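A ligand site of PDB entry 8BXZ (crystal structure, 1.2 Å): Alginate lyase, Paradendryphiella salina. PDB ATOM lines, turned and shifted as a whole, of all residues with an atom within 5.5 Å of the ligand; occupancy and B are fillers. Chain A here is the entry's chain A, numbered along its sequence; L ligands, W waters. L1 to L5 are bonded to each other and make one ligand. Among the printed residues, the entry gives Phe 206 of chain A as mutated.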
ATOM      1  N   LYS A  20      -7.874 -21.116  28.085  1.00  0.00           N
ATOM      2  CA  LYS A  20      -8.801 -20.235  28.762  1.00  0.00           C
ATOM      3  C   LYS A  20      -9.092 -19.084  27.810  1.00  0.00           C
ATOM      4  O   LYS A  20      -8.304 -18.787  26.909  1.00  0.00           O
ATOM      5  CB  LYS A  20      -8.250 -19.708  30.094  1.00  0.00           C
ATOM      6  CG  LYS A  20      -7.019 -18.833  29.929  1.00  0.00           C
ATOM      7  CD  LYS A  20      -6.530 -18.239  31.242  1.00  0.00           C
ATOM      8  CE  LYS A  20      -5.222 -17.501  31.037  1.00  0.00           C
ATOM      9  NZ  LYS A  20      -4.742 -16.824  32.270  1.00  0.00           N
ATOM     10  N   GLN A  22      -9.568 -15.037  27.545  1.00  0.00           N
ATOM     11  CA  GLN A  22      -9.361 -13.708  28.114  1.00  0.00           C
ATOM     12  C   GLN A  22     -10.212 -12.719  27.333  1.00  0.00           C
ATOM     13  O   GLN A  22     -10.091 -12.624  26.120  1.00  0.00           O
ATOM     14  CB  GLN A  22      -7.888 -13.335  27.997  1.00  0.00           C
ATOM     15  CG  GLN A  22      -6.950 -14.296  28.705  1.00  0.00           C
ATOM     16  CD  GLN A  22      -5.511 -13.969  28.441  1.00  0.00           C
ATOM     17  OE1 GLN A  22      -5.095 -13.869  27.291  1.00  0.00           O
ATOM     18  NE2 GLN A  22      -4.736 -13.763  29.491  1.00  0.00           N
ATOM     19  N   SER A  26      -6.821  -8.963  29.596  1.00  0.00           N
ATOM     20  CA  SER A  26      -6.109 -10.185  29.958  1.00  0.00           C
ATOM     21  C   SER A  26      -6.758 -10.915  31.122  1.00  0.00           C
ATOM     22  O   SER A  26      -6.414 -12.080  31.362  1.00  0.00           O
ATOM     23  CB  SER A  26      -4.661  -9.865  30.285  1.00  0.00           C
ATOM     24  OG  SER A  26      -3.976  -9.485  29.114  1.00  0.00           O
ATOM     25  N   ALA A  27      -7.686 -10.289  31.836  1.00  0.00           N
ATOM     26  CA  ALA A  27      -8.368 -10.992  32.909  1.00  0.00           C
ATOM     27  C   ALA A  27      -9.186 -12.153  32.347  1.00  0.00           C
ATOM     28  O   ALA A  27      -9.684 -12.118  31.216  1.00  0.00           O
ATOM     29  CB  ALA A  27      -9.251 -10.038  33.704  1.00  0.00           C
ATOM     30  N   LEU A  28      -9.339 -13.185  33.163  1.00  0.00           N
ATOM     31  CA  LEU A  28     -10.025 -14.401  32.758  1.00  0.00           C
ATOM     32  C   LEU A  28     -11.495 -14.114  32.494  1.00  0.00           C
ATOM     33  O   LEU A  28     -12.179 -13.489  33.313  1.00  0.00           O
ATOM     34  CB  LEU A  28      -9.907 -15.419  33.886  1.00  0.00           C
ATOM     35  CG  LEU A  28     -10.663 -16.727  33.759  1.00  0.00           C
ATOM     36  CD1 LEU A  28     -10.099 -17.539  32.616  1.00  0.00           C
ATOM     37  CD2 LEU A  28     -10.588 -17.524  35.045  1.00  0.00           C
ATOM     38  N   SER A  60      -6.138  -2.195  22.593  1.00  0.00           N
ATOM     39  CA  SER A  60      -5.455  -3.231  23.348  1.00  0.00           C
ATOM     40  C   SER A  60      -6.399  -4.147  24.105  1.00  0.00           C
ATOM     41  O   SER A  60      -5.946  -4.946  24.920  1.00  0.00           O
ATOM     42  CB  SER A  60      -4.376  -2.653  24.266  1.00  0.00           C
ATOM     43  OG  SER A  60      -3.412  -1.954  23.501  1.00  0.00           O
ATOM     44  N   ARG A  62      -8.984  -7.429  24.078  1.00  0.00           N
ATOM     45  CA  ARG A  62      -8.819  -8.712  23.420  1.00  0.00           C
ATOM     46  C   ARG A  62     -10.024  -9.601  23.691  1.00  0.00           C
ATOM     47  O   ARG A  62     -10.734  -9.448  24.686  1.00  0.00           O
ATOM     48  CB  ARG A  62      -7.548  -9.419  23.903  1.00  0.00           C
ATOM     49  CG  ARG A  62      -7.621  -9.885  25.311  1.00  0.00           C
ATOM     50  CD  ARG A  62      -6.260 -10.306  25.813  1.00  0.00           C
ATOM     51  NE  ARG A  62      -5.410  -9.141  26.058  1.00  0.00           N
ATOM     52  CZ  ARG A  62      -4.201  -8.942  25.565  1.00  0.00           C
ATOM     53  NH1 ARG A  62      -3.679  -9.723  24.644  1.00  0.00           N
ATOM     54  NH2 ARG A  62      -3.479  -7.912  26.020  1.00  0.00           N
ATOM     55  N   GLU A  64      -9.390 -13.544  23.406  1.00  0.00           N
ATOM     56  CA  GLU A  64      -8.297 -14.397  23.002  1.00  0.00           C
ATOM     57  C   GLU A  64      -8.247 -15.655  23.840  1.00  0.00           C
ATOM     58  O   GLU A  64      -8.401 -15.603  25.063  1.00  0.00           O
ATOM     59  CB  GLU A  64      -6.937 -13.709  23.214  1.00  0.00           C
ATOM     60  CG  GLU A  64      -6.283 -13.073  22.038  1.00  0.00           C
ATOM     61  CD  GLU A  64      -4.838 -12.701  22.326  1.00  0.00           C
ATOM     62  OE1 GLU A  64      -4.562 -12.108  23.390  1.00  0.00           O
ATOM     63  OE2 GLU A  64      -3.985 -12.980  21.453  1.00  0.00           O
ATOM     64  N   ARG A  66      -5.860 -18.476  25.422  1.00  0.00           N
ATOM     65  CA  ARG A  66      -4.529 -18.534  25.999  1.00  0.00           C
ATOM     66  C   ARG A  66      -4.259 -19.984  26.385  1.00  0.00           C
ATOM     67  O   ARG A  66      -5.041 -20.597  27.127  1.00  0.00           O
ATOM     68  CB  ARG A  66      -4.493 -17.625  27.234  1.00  0.00           C
ATOM     69  CG  ARG A  66      -3.128 -17.353  27.815  1.00  0.00           C
ATOM     70  CD  ARG A  66      -2.521 -18.530  28.581  1.00  0.00           C
ATOM     71  NE  ARG A  66      -1.502 -18.040  29.498  1.00  0.00           N
ATOM     72  CZ  ARG A  66      -0.410 -18.685  29.864  1.00  0.00           C
ATOM     73  NH1 ARG A  66      -0.144 -19.907  29.438  1.00  0.00           N
ATOM     74  NH2 ARG A  66       0.456 -18.077  30.675  1.00  0.00           N
ATOM     75  N   GLU A  75      -1.987 -22.481  33.814  1.00  0.00           N
ATOM     76  CA  GLU A  75      -1.287 -21.885  32.688  1.00  0.00           C
ATOM     77  C   GLU A  75      -0.027 -22.669  32.336  1.00  0.00           C
ATOM     78  O   GLU A  75       0.749 -23.051  33.210  1.00  0.00           O
ATOM     79  CB  GLU A  75      -0.892 -20.450  33.058  1.00  0.00           C
ATOM     80  CG  GLU A  75      -2.033 -19.419  33.014  1.00  0.00           C
ATOM     81  CD  GLU A  75      -2.992 -19.460  34.208  1.00  0.00           C
ATOM     82  OE1 GLU A  75      -2.708 -20.140  35.207  1.00  0.00           O
ATOM     83  OE2 GLU A  75      -4.039 -18.766  34.123  1.00  0.00           O
ATOM     84  N   GLU A 103      -5.358  -2.873  13.047  1.00  0.00           N
ATOM     85  CA  GLU A 103      -4.486  -4.032  13.150  1.00  0.00           C
ATOM     86  C   GLU A 103      -5.133  -4.964  14.151  1.00  0.00           C
ATOM     87  O   GLU A 103      -5.583  -4.505  15.203  1.00  0.00           O
ATOM     88  CB  GLU A 103      -3.060  -3.664  13.600  1.00  0.00           C
ATOM     89  CG  GLU A 103      -2.186  -4.920  13.810  1.00  0.00           C
ATOM     90  CD  GLU A 103      -0.723  -4.653  14.157  1.00  0.00           C
ATOM     91  OE1 GLU A 103      -0.363  -3.526  14.549  1.00  0.00           O
ATOM     92  OE2 GLU A 103       0.074  -5.615  14.065  1.00  0.00           O
ATOM     93  N   GLN A 108      -0.511 -15.689  18.453  1.00  0.00           N
ATOM     94  CA  GLN A 108       0.713 -15.252  19.088  1.00  0.00           C
ATOM     95  C   GLN A 108       1.480 -16.427  19.695  1.00  0.00           C
ATOM     96  O   GLN A 108       0.912 -17.473  20.013  1.00  0.00           O
ATOM     97  CB  GLN A 108       0.456 -14.289  20.254  1.00  0.00           C
ATOM     98  CG  GLN A 108      -0.443 -13.127  19.928  1.00  0.00           C
ATOM     99  CD  GLN A 108      -0.406 -12.029  20.961  1.00  0.00           C
ATOM    100  OE1 GLN A 108       0.644 -11.413  21.196  1.00  0.00           O
ATOM    101  NE2 GLN A 108      -1.550 -11.758  21.594  1.00  0.00           N
ATOM    102  N   HIS A 110       3.720 -15.981  23.148  1.00  0.00           N
ATOM    103  CA  HIS A 110       3.951 -14.972  24.172  1.00  0.00           C
ATOM    104  C   HIS A 110       4.593 -15.652  25.359  1.00  0.00           C
ATOM    105  O   HIS A 110       4.467 -16.854  25.543  1.00  0.00           O
ATOM    106  CB  HIS A 110       2.607 -14.335  24.567  1.00  0.00           C
ATOM    107  CG  HIS A 110       2.718 -12.975  25.181  1.00  0.00           C
ATOM    108  ND1 HIS A 110       3.247 -12.751  26.437  1.00  0.00           N
ATOM    109  CD2 HIS A 110       2.331 -11.764  24.717  1.00  0.00           C
ATOM    110  CE1 HIS A 110       3.197 -11.452  26.707  1.00  0.00           C
ATOM    111  NE2 HIS A 110       2.660 -10.833  25.681  1.00  0.00           N
ATOM    112  N   GLU A 113       7.167 -12.142  29.603  1.00  0.00           N
ATOM    113  CA  GLU A 113       7.628 -10.774  29.418  1.00  0.00           C
ATOM    114  C   GLU A 113       7.149 -10.091  28.143  1.00  0.00           C
ATOM    115  O   GLU A 113       6.963  -8.878  28.154  1.00  0.00           O
ATOM    116  CB  GLU A 113       9.166 -10.726  29.480  1.00  0.00           C
ATOM    117  CG  GLU A 113       9.688 -10.999  30.897  1.00  0.00           C
ATOM    118  CD  GLU A 113      11.198 -10.943  31.026  1.00  0.00           C
ATOM    119  OE1 GLU A 113      11.835 -10.111  30.340  1.00  0.00           O
ATOM    120  OE2 GLU A 113      11.748 -11.729  31.823  1.00  0.00           O
ATOM    121  N   ALA A 114       6.950 -10.820  27.038  1.00  0.00           N
ATOM    122  CA  ALA A 114       6.694 -10.148  25.766  1.00  0.00           C
ATOM    123  C   ALA A 114       6.186 -11.141  24.732  1.00  0.00           C
ATOM    124  O   ALA A 114       6.306 -12.360  24.918  1.00  0.00           O
ATOM    125  CB  ALA A 114       7.964  -9.488  25.225  1.00  0.00           C
ATOM    126  N   PRO A 115       5.642 -10.655  23.608  1.00  0.00           N
ATOM    127  CA  PRO A 115       5.281 -11.542  22.498  1.00  0.00           C
ATOM    128  C   PRO A 115       6.487 -11.854  21.624  1.00  0.00           C
ATOM    129  O   PRO A 115       7.085 -10.985  20.988  1.00  0.00           O
ATOM    130  CB  PRO A 115       4.230 -10.727  21.729  1.00  0.00           C
ATOM    131  CG  PRO A 115       4.590  -9.335  21.993  1.00  0.00           C
ATOM    132  CD  PRO A 115       5.165  -9.283  23.383  1.00  0.00           C
ATOM    133  N   ARG A 118       3.716 -12.217  16.838  1.00  0.00           N
ATOM    134  CA  ARG A 118       2.323 -11.908  16.533  1.00  0.00           C
ATOM    135  C   ARG A 118       2.097 -12.105  15.046  1.00  0.00           C
ATOM    136  O   ARG A 118       2.850 -11.578  14.217  1.00  0.00           O
ATOM    137  CB  ARG A 118       1.960 -10.469  16.897  1.00  0.00           C
ATOM    138  CG  ARG A 118       2.121 -10.110  18.354  1.00  0.00           C
ATOM    139  CD  ARG A 118       1.607  -8.714  18.665  1.00  0.00           C
ATOM    140  NE  ARG A 118       2.245  -7.685  17.853  1.00  0.00           N
ATOM    141  CZ  ARG A 118       1.707  -7.130  16.774  1.00  0.00           C
ATOM    142  NH1 ARG A 118       0.481  -7.398  16.391  1.00  0.00           N
ATOM    143  NH2 ARG A 118       2.456  -6.303  16.043  1.00  0.00           N
ATOM    144  N   THR A 139       5.206 -10.418  13.126  1.00  0.00           N
ATOM    145  CA  THR A 139       6.118  -9.572  13.881  1.00  0.00           C
ATOM    146  C   THR A 139       6.799 -10.467  14.898  1.00  0.00           C
ATOM    147  O   THR A 139       6.138 -10.986  15.810  1.00  0.00           O
ATOM    148  CB  THR A 139       5.389  -8.429  14.570  1.00  0.00           C
ATOM    149  OG1 THR A 139       4.743  -7.583  13.618  1.00  0.00           O
ATOM    150  CG2 THR A 139       6.379  -7.573  15.373  1.00  0.00           C
ATOM    151  N   ARG A 141       9.793 -10.724  17.782  1.00  0.00           N
ATOM    152  CA  ARG A 141      10.725  -9.999  18.628  1.00  0.00           C
ATOM    153  C   ARG A 141      12.037 -10.750  18.731  1.00  0.00           C
ATOM    154  O   ARG A 141      12.067 -11.930  19.108  1.00  0.00           O
ATOM    155  CB  ARG A 141      10.177  -9.750  20.031  1.00  0.00           C
ATOM    156  CG  ARG A 141       9.352  -8.497  20.142  1.00  0.00           C
ATOM    157  CD  ARG A 141       8.991  -8.231  21.594  1.00  0.00           C
ATOM    158  NE  ARG A 141       8.387  -6.915  21.764  1.00  0.00           N
ATOM    159  CZ  ARG A 141       9.061  -5.777  21.867  1.00  0.00           C
ATOM    160  NH1 ARG A 141      10.383  -5.753  21.815  1.00  0.00           N
ATOM    161  NH2 ARG A 141       8.399  -4.638  22.013  1.00  0.00           N
ATOM    162  N   ASP A 146      12.015  -1.059  21.794  1.00  0.00           N
ATOM    163  CA  ASP A 146      10.962  -0.561  20.915  1.00  0.00           C
ATOM    164  C   ASP A 146      11.441  -0.124  19.535  1.00  0.00           C
ATOM    165  O   ASP A 146      10.607   0.050  18.630  1.00  0.00           O
ATOM    166  CB  ASP A 146      10.211   0.579  21.601  1.00  0.00           C
ATOM    167  CG  ASP A 146       9.641   0.159  22.939  1.00  0.00           C
ATOM    168  OD1 ASP A 146       9.082  -0.962  22.999  1.00  0.00           O
ATOM    169  OD2 ASP A 146       9.784   0.919  23.913  1.00  0.00           O
ATOM    170  N   PHE A 151      12.729  -6.084  16.071  1.00  0.00           N
ATOM    171  CA  PHE A 151      11.664  -6.796  15.383  1.00  0.00           C
ATOM    172  C   PHE A 151      12.122  -7.295  14.025  1.00  0.00           C
ATOM    173  O   PHE A 151      12.950  -6.670  13.365  1.00  0.00           O
ATOM    174  CB  PHE A 151      10.460  -5.891  15.163  1.00  0.00           C
ATOM    175  CG  PHE A 151       9.968  -5.228  16.404  1.00  0.00           C
ATOM    176  CD1 PHE A 151       9.136  -5.885  17.289  1.00  0.00           C
ATOM    177  CD2 PHE A 151      10.361  -3.932  16.688  1.00  0.00           C
ATOM    178  CE1 PHE A 151       8.687  -5.239  18.441  1.00  0.00           C
ATOM    179  CE2 PHE A 151       9.941  -3.297  17.827  1.00  0.00           C
ATOM    180  CZ  PHE A 151       9.091  -3.943  18.706  1.00  0.00           C
ATOM    181  N   LYS A 153       9.722  -8.051  10.831  1.00  0.00           N
ATOM    182  CA  LYS A 153       8.348  -7.956  10.369  1.00  0.00           C
ATOM    183  C   LYS A 153       8.281  -8.401   8.914  1.00  0.00           C
ATOM    184  O   LYS A 153       9.120  -8.016   8.103  1.00  0.00           O
ATOM    185  CB  LYS A 153       7.806  -6.537  10.579  1.00  0.00           C
ATOM    186  CG  LYS A 153       7.709  -6.148  12.074  1.00  0.00           C
ATOM    187  CD  LYS A 153       7.455  -4.654  12.317  1.00  0.00           C
ATOM    188  CE  LYS A 153       5.983  -4.321  12.257  1.00  0.00           C
ATOM    189  NZ  LYS A 153       5.232  -4.701  13.476  1.00  0.00           N
ATOM    190  N   TYR A 200       3.928 -19.574  25.499  1.00  0.00           N
ATOM    191  CA  TYR A 200       2.644 -20.207  25.291  1.00  0.00           C
ATOM    192  C   TYR A 200       2.028 -19.628  24.021  1.00  0.00           C
ATOM    193  O   TYR A 200       2.361 -18.523  23.598  1.00  0.00           O
ATOM    194  CB  TYR A 200       1.712 -19.986  26.485  1.00  0.00           C
ATOM    195  CG  TYR A 200       1.509 -18.528  26.865  1.00  0.00           C
ATOM    196  CD1 TYR A 200       2.359 -17.915  27.777  1.00  0.00           C
ATOM    197  CD2 TYR A 200       0.465 -17.771  26.355  1.00  0.00           C
ATOM    198  CE1 TYR A 200       2.188 -16.596  28.150  1.00  0.00           C
ATOM    199  CE2 TYR A 200       0.293 -16.442  26.733  1.00  0.00           C
ATOM    200  CZ  TYR A 200       1.148 -15.865  27.627  1.00  0.00           C
ATOM    201  OH  TYR A 200       0.926 -14.538  27.969  1.00  0.00           O
ATOM    202  N   LYS A 202      -1.300 -18.138  21.863  1.00  0.00           N
ATOM    203  CA  LYS A 202      -2.578 -17.432  21.977  1.00  0.00           C
ATOM    204  C   LYS A 202      -3.199 -17.372  20.594  1.00  0.00           C
ATOM    205  O   LYS A 202      -2.508 -17.426  19.576  1.00  0.00           O
ATOM    206  CB  LYS A 202      -2.411 -15.999  22.483  1.00  0.00           C
ATOM    207  CG  LYS A 202      -1.525 -15.847  23.704  1.00  0.00           C
ATOM    208  CD  LYS A 202      -1.624 -14.458  24.282  1.00  0.00           C
ATOM    209  CE  LYS A 202      -2.781 -14.356  25.256  1.00  0.00           C
ATOM    210  NZ  LYS A 202      -3.139 -12.950  25.644  1.00  0.00           N
ATOM    211  N   PHE A 206      -6.978  -9.593  19.092  1.00  0.00           N
ATOM    212  CA  PHE A 206      -6.391  -8.633  20.012  1.00  0.00           C
ATOM    213  C   PHE A 206      -6.214  -7.360  19.194  1.00  0.00           C
ATOM    214  O   PHE A 206      -5.515  -7.357  18.176  1.00  0.00           O
ATOM    215  CB  PHE A 206      -5.113  -9.244  20.600  1.00  0.00           C
ATOM    216  CG  PHE A 206      -4.170  -8.278  21.257  1.00  0.00           C
ATOM    217  CD1 PHE A 206      -4.606  -7.344  22.169  1.00  0.00           C
ATOM    218  CD2 PHE A 206      -2.819  -8.400  21.029  1.00  0.00           C
ATOM    219  CE1 PHE A 206      -3.718  -6.486  22.776  1.00  0.00           C
ATOM    220  CE2 PHE A 206      -1.922  -7.552  21.637  1.00  0.00           C
ATOM    221  CZ  PHE A 206      -2.387  -6.599  22.524  1.00  0.00           C
ATOM    222  N   ASN A 208      -5.212  -3.772  17.984  1.00  0.00           N
ATOM    223  CA  ASN A 208      -4.014  -2.943  18.110  1.00  0.00           C
ATOM    224  C   ASN A 208      -4.187  -1.605  17.411  1.00  0.00           C
ATOM    225  O   ASN A 208      -4.487  -1.551  16.214  1.00  0.00           O
ATOM    226  CB  ASN A 208      -2.814  -3.660  17.509  1.00  0.00           C
ATOM    227  CG  ASN A 208      -2.735  -5.115  17.933  1.00  0.00           C
ATOM    228  OD1 ASN A 208      -2.749  -6.025  17.099  1.00  0.00           O
ATOM    229  ND2 ASN A 208      -2.672  -5.349  19.236  1.00  0.00           N
ATOM    230  N   ASN A 209      -3.970  -0.526  18.151  1.00  0.00           N
ATOM    231  CA  ASN A 209      -3.935   0.830  17.598  1.00  0.00           C
ATOM    232  C   ASN A 209      -5.159   1.204  16.754  1.00  0.00           C
ATOM    233  O   ASN A 209      -5.008   1.806  15.690  1.00  0.00           O
ATOM    234  CB  ASN A 209      -2.659   1.047  16.793  1.00  0.00           C
ATOM    235  CG  ASN A 209      -1.407   0.705  17.580  1.00  0.00           C
ATOM    236  OD1 ASN A 209      -1.278   1.045  18.742  1.00  0.00           O
ATOM    237  ND2 ASN A 209      -0.491   0.013  16.927  1.00  0.00           N
HETATM  238  C1  LIG L   1      -3.899 -13.425  33.807  1.00  0.00           C
HETATM  239  C2  LIG L   1      -3.448 -11.986  33.520  1.00  0.00           C
HETATM  240  O1  LIG L   1      -3.808 -11.129  34.616  1.00  0.00           O
HETATM  241  C3  LIG L   1      -1.987 -11.818  33.243  1.00  0.00           C
HETATM  242  O2  LIG L   1      -1.240 -11.937  34.489  1.00  0.00           O
HETATM  243  C4  LIG L   1      -1.480 -12.828  32.256  1.00  0.00           C
HETATM  244  O3  LIG L   1      -1.936 -12.622  30.928  1.00  0.00           O
HETATM  245  C5  LIG L   1      -2.236 -14.127  32.340  1.00  0.00           C
HETATM  246  O4  LIG L   1      -2.809 -14.437  33.634  1.00  0.00           O
HETATM  247  C6  LIG L   1      -1.520 -15.268  31.711  1.00  0.00           C
HETATM  248  O5  LIG L   1      -0.258 -15.412  31.638  1.00  0.00           O
HETATM  249  O6  LIG L   1      -2.321 -16.063  31.190  1.00  0.00           O
HETATM  250  O7  LIG L   1      -4.404 -13.625  35.038  1.00  0.00           O
HETATM  251  C1  LG2 L   2      -1.042 -11.884  30.151  1.00  0.00           C
HETATM  252  C2  LG2 L   2      -1.304 -12.124  28.694  1.00  0.00           C
HETATM  253  O1  LG2 L   2      -2.701 -11.888  28.397  1.00  0.00           O
HETATM  254  C3  LG2 L   2      -0.402 -11.242  27.900  1.00  0.00           C
HETATM  255  O2  LG2 L   2      -0.784 -11.364  26.509  1.00  0.00           O
HETATM  256  C4  LG2 L   2      -0.428  -9.803  28.354  1.00  0.00           C
HETATM  257  O3  LG2 L   2       0.763  -9.181  27.911  1.00  0.00           O
HETATM  258  C5  LG2 L   2      -0.344  -9.643  29.869  1.00  0.00           C
HETATM  259  O4  LG2 L   2      -1.296 -10.497  30.520  1.00  0.00           O
HETATM  260  C6  LG2 L   2      -0.671  -8.245  30.261  1.00  0.00           C
HETATM  261  O5  LG2 L   2       0.234  -7.511  30.736  1.00  0.00           O
HETATM  262  O6  LG2 L   2      -1.858  -7.830  30.126  1.00  0.00           O
HETATM  263  C1  LG3 L   3       0.599  -8.238  26.897  1.00  0.00           C
HETATM  264  C2  LG3 L   3       1.796  -7.326  26.758  1.00  0.00           C
HETATM  265  O1  LG3 L   3       2.974  -8.130  26.513  1.00  0.00           O
HETATM  266  C3  LG3 L   3       1.621  -6.386  25.610  1.00  0.00           C
HETATM  267  O2  LG3 L   3       2.795  -5.553  25.489  1.00  0.00           O
HETATM  268  C4  LG3 L   3       1.345  -7.071  24.298  1.00  0.00           C
HETATM  269  O3  LG3 L   3       0.873  -6.037  23.434  1.00  0.00           O
HETATM  270  C5  LG3 L   3       0.214  -8.099  24.511  1.00  0.00           C
HETATM  271  O4  LG3 L   3       0.425  -9.005  25.650  1.00  0.00           O
HETATM  272  C6  LG3 L   3       0.052  -9.133  23.467  1.00  0.00           C
HETATM  273  O5  LG3 L   3       0.905  -9.306  22.562  1.00  0.00           O
HETATM  274  O6  LG3 L   3      -0.982  -9.850  23.581  1.00  0.00           O
HETATM  275  C1  LG4 L   4       1.497  -5.964  22.156  1.00  0.00           C
HETATM  276  C2  LG4 L   4       0.890  -4.871  21.312  1.00  0.00           C
HETATM  277  O1  LG4 L   4       0.977  -3.609  22.001  1.00  0.00           O
HETATM  278  C3  LG4 L   4       1.607  -4.739  20.014  1.00  0.00           C
HETATM  279  O2  LG4 L   4       1.026  -3.633  19.265  1.00  0.00           O
HETATM  280  C4  LG4 L   4       3.105  -4.554  20.172  1.00  0.00           C
HETATM  281  O3  LG4 L   4       3.725  -4.710  18.904  1.00  0.00           O
HETATM  282  C5  LG4 L   4       3.614  -5.678  21.050  1.00  0.00           C
HETATM  283  O4  LG4 L   4       2.934  -5.687  22.339  1.00  0.00           O
HETATM  284  C6  LG4 L   4       5.063  -5.568  21.347  1.00  0.00           C
HETATM  285  O5  LG4 L   4       5.466  -4.889  22.321  1.00  0.00           O
HETATM  286  O6  LG4 L   4       5.867  -6.207  20.618  1.00  0.00           O
HETATM  287  C1  LG5 L   5       4.633  -3.691  18.568  1.00  0.00           C
HETATM  288  C2  LG5 L   5       5.353  -4.038  17.284  1.00  0.00           C
HETATM  289  O1  LG5 L   5       4.368  -4.327  16.265  1.00  0.00           O
HETATM  290  C3  LG5 L   5       6.188  -2.904  16.827  1.00  0.00           C
HETATM  291  O2  LG5 L   5       6.766  -3.240  15.544  1.00  0.00           O
HETATM  292  C4  LG5 L   5       5.382  -1.645  16.681  1.00  0.00           C
HETATM  293  O3  LG5 L   5       6.224  -0.540  16.376  1.00  0.00           O
HETATM  294  C5  LG5 L   5       4.588  -1.331  17.961  1.00  0.00           C
HETATM  295  O4  LG5 L   5       3.832  -2.475  18.441  1.00  0.00           O
HETATM  296  C6  LG5 L   5       3.566  -0.270  17.733  1.00  0.00           C
HETATM  297  O5  LG5 L   5       3.808   0.907  18.097  1.00  0.00           O
HETATM  298  O6  LG5 L   5       2.449  -0.535  17.196  1.00  0.00           O
HETATM  299  O   HOH W   1      -0.903  -3.432  24.010  1.00  0.00           O
HETATM  300  O   HOH W   2       8.617  -1.595  14.424  1.00  0.00           O
HETATM  301  O   HOH W   3      -2.161  -3.046  21.064  1.00  0.00           O
HETATM  302  O   HOH W   4       2.276  -0.800  13.867  1.00  0.00           O
HETATM  303  O   HOH W   5      -6.582 -14.680  32.480  1.00  0.00           O
HETATM  304  O   HOH W   6       2.502   2.894  17.402  1.00  0.00           O
HETATM  305  O   HOH W   7       1.325 -10.504  33.507  1.00  0.00           O
HETATM  306  O   HOH W   8      -6.333 -15.805  34.927  1.00  0.00           O
HETATM  307  O   HOH W   9       4.991  -7.543  18.441  1.00  0.00           O
HETATM  308  O   HOH W  10       5.513  -7.043  26.894  1.00  0.00           O
HETATM  309  O   HOH W  11       7.939  -0.199  18.746  1.00  0.00           O
HETATM  310  O   HOH W  12      -3.306  -6.276  28.684  1.00  0.00           O
HETATM  311  O   HOH W  13       1.672  -3.214  16.554  1.00  0.00           O
HETATM  312  O   HOH W  14       1.962 -13.959  30.434  1.00  0.00           O
HETATM  313  O   HOH W  15       3.810  -3.013  23.598  1.00  0.00           O
HETATM  314  O   HOH W  16       6.374  -5.935  24.685  1.00  0.00           O
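Water W1 lies within hydrogen-bond range of O1 of LG4 L4 (2.8 Å) and OG of Ser 60 (3.0 Å).
Water W10 lies within hydrogen-bond range of the backbone carbonyl oxygen of Glu 113 (2.7 Å) and an oxygen (O1) of LG3 L3 (2.8 Å).
Water W13 lies within hydrogen-bond range of an oxygen (O2) of LG4 L4 (2.8 Å), the side-chain carboxylate of Glu 103 (2.9 Å) and the guanidinium group of Arg 118 (3.2 Å).
Water W11 bridges the backbone carbonyl oxygen of Asp 146 (2.7 Å) and an oxygen (O3) of LG5 L5 (2.9 Å).
Water W5 lies within hydrogen-bond range of the side-chain amino group (NZ) of Lys 20, the backbone carbonyl oxygen (O) of Ser 26 and the backbone NH (N) of Leu 28.
Water W3 lies within hydrogen-bond range of the side-chain hydroxyl (OG) of Ser 60 (2.9 Å), the side-chain amide nitrogen (ND2) of Asn 208 (3.0 Å) and an oxygen (O1) of LG4 L4 (3.3 Å).
CG of Glu 75 touches O6 of LIG L1, 3.8 Å away.
CG of Pro 115 touches O6 of LG4 L4, 3.6 Å away.
CG2 of Thr 139 touches O1 of LG5 L5, at 3.9 Å.
Phe 151 touches the ligand.
OH of Tyr 200 touches C2 of LG2 L2, 3.4 Å away.
CE2 of Phe 206 touches C6 of LG3 L3 (3.1 Å).
Hydrophobic or aromatic side chains within 4 Å of the ligand: His 110, Pro 115, Phe 151 and Phe 206.
Along chain A the residues within 4 Å of the ligand span positions 20 to 209.
The nearest printed residue that does not touch the ligand is Asn 208 (4.1 Å).
OE1 of Gln 108 sits close to O5 of LG3 L3 (2.5 Å).
The guanidinium group (NE) of Arg 66 lies within salt-bridge range of an oxygen (O6) of LIG L1, at 2.7 Å.
The side-chain amino group (NZ) of Lys 20 is in salt-bridge range of an oxygen (O6) of LIG L1 (2.8 Å).
The guanidinium group of Arg 118 sits at hydrogen-bond distance from an oxygen (O1) of LG5 L5 (2.8 Å).
The side-chain hydroxyl (OG) of Ser 26 lies within hydrogen-bond range of an oxygen (O1) of LG2 L2, at 2.8 Å.
A ring nitrogen (NE2) of His 110 is in hydrogen-bond range of an oxygen (O1) of LG3 L3 (2.8 Å).
The guanidinium group (NE) of Arg 141 is in salt-bridge range of an oxygen (O6) of LG4 L4 (2.9 Å).
The guanidinium group (NH1) of Arg 62 lies within salt-bridge range of an oxygen (O6) of LG3 L3 (2.9 Å).
The side-chain amino group of Lys 153 sits at hydrogen-bond distance from an oxygen (O1) of LG5 L5 (2.9 Å).
An oxygen (O2) of LG2 L2 lies within hydrogen-bond range of the side-chain amino group (NZ) of Lys 202, 3.0 Å away.
The side-chain amide nitrogen (NE2) of Gln 22 sits at hydrogen-bond distance from an oxygen (O1) of LG2 L2 (3.0 Å).
ND2 of Asn 209 is in hydrogen-bond range of O6 of LG5 L5, 3.0 Å away.
The side-chain carboxylate (OE2) of Glu 64 sits at hydrogen-bond distance from the side-chain amide nitrogen (NE2) of Gln 108, at 2.7 Å.
The backbone NH (N) of Arg 66 sits at hydrogen-bond distance from the backbone carbonyl oxygen (O) of Lys 20 (2.9 Å).
The side-chain hydroxyl of Ser 26 lies within hydrogen-bond range of the guanidinium group of Arg 62.
O of Ser 26 lies within hydrogen-bond range of NE2 of Gln 22, 3.0 Å away.
OE1 of Glu 64 lies within salt-bridge range of NH1 of Arg 62 (2.8 Å).
NZ of Lys 153 lies within hydrogen-bond range of OG1 of Thr 139 (2.9 Å).
NZ of Lys 202 lies within salt-bridge range of OE1 of Glu 64 (2.8 Å).
The backbone carbonyl oxygen of Phe 206 lies close to the side-chain amide oxygen of Asn 208, at 3.3 Å.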
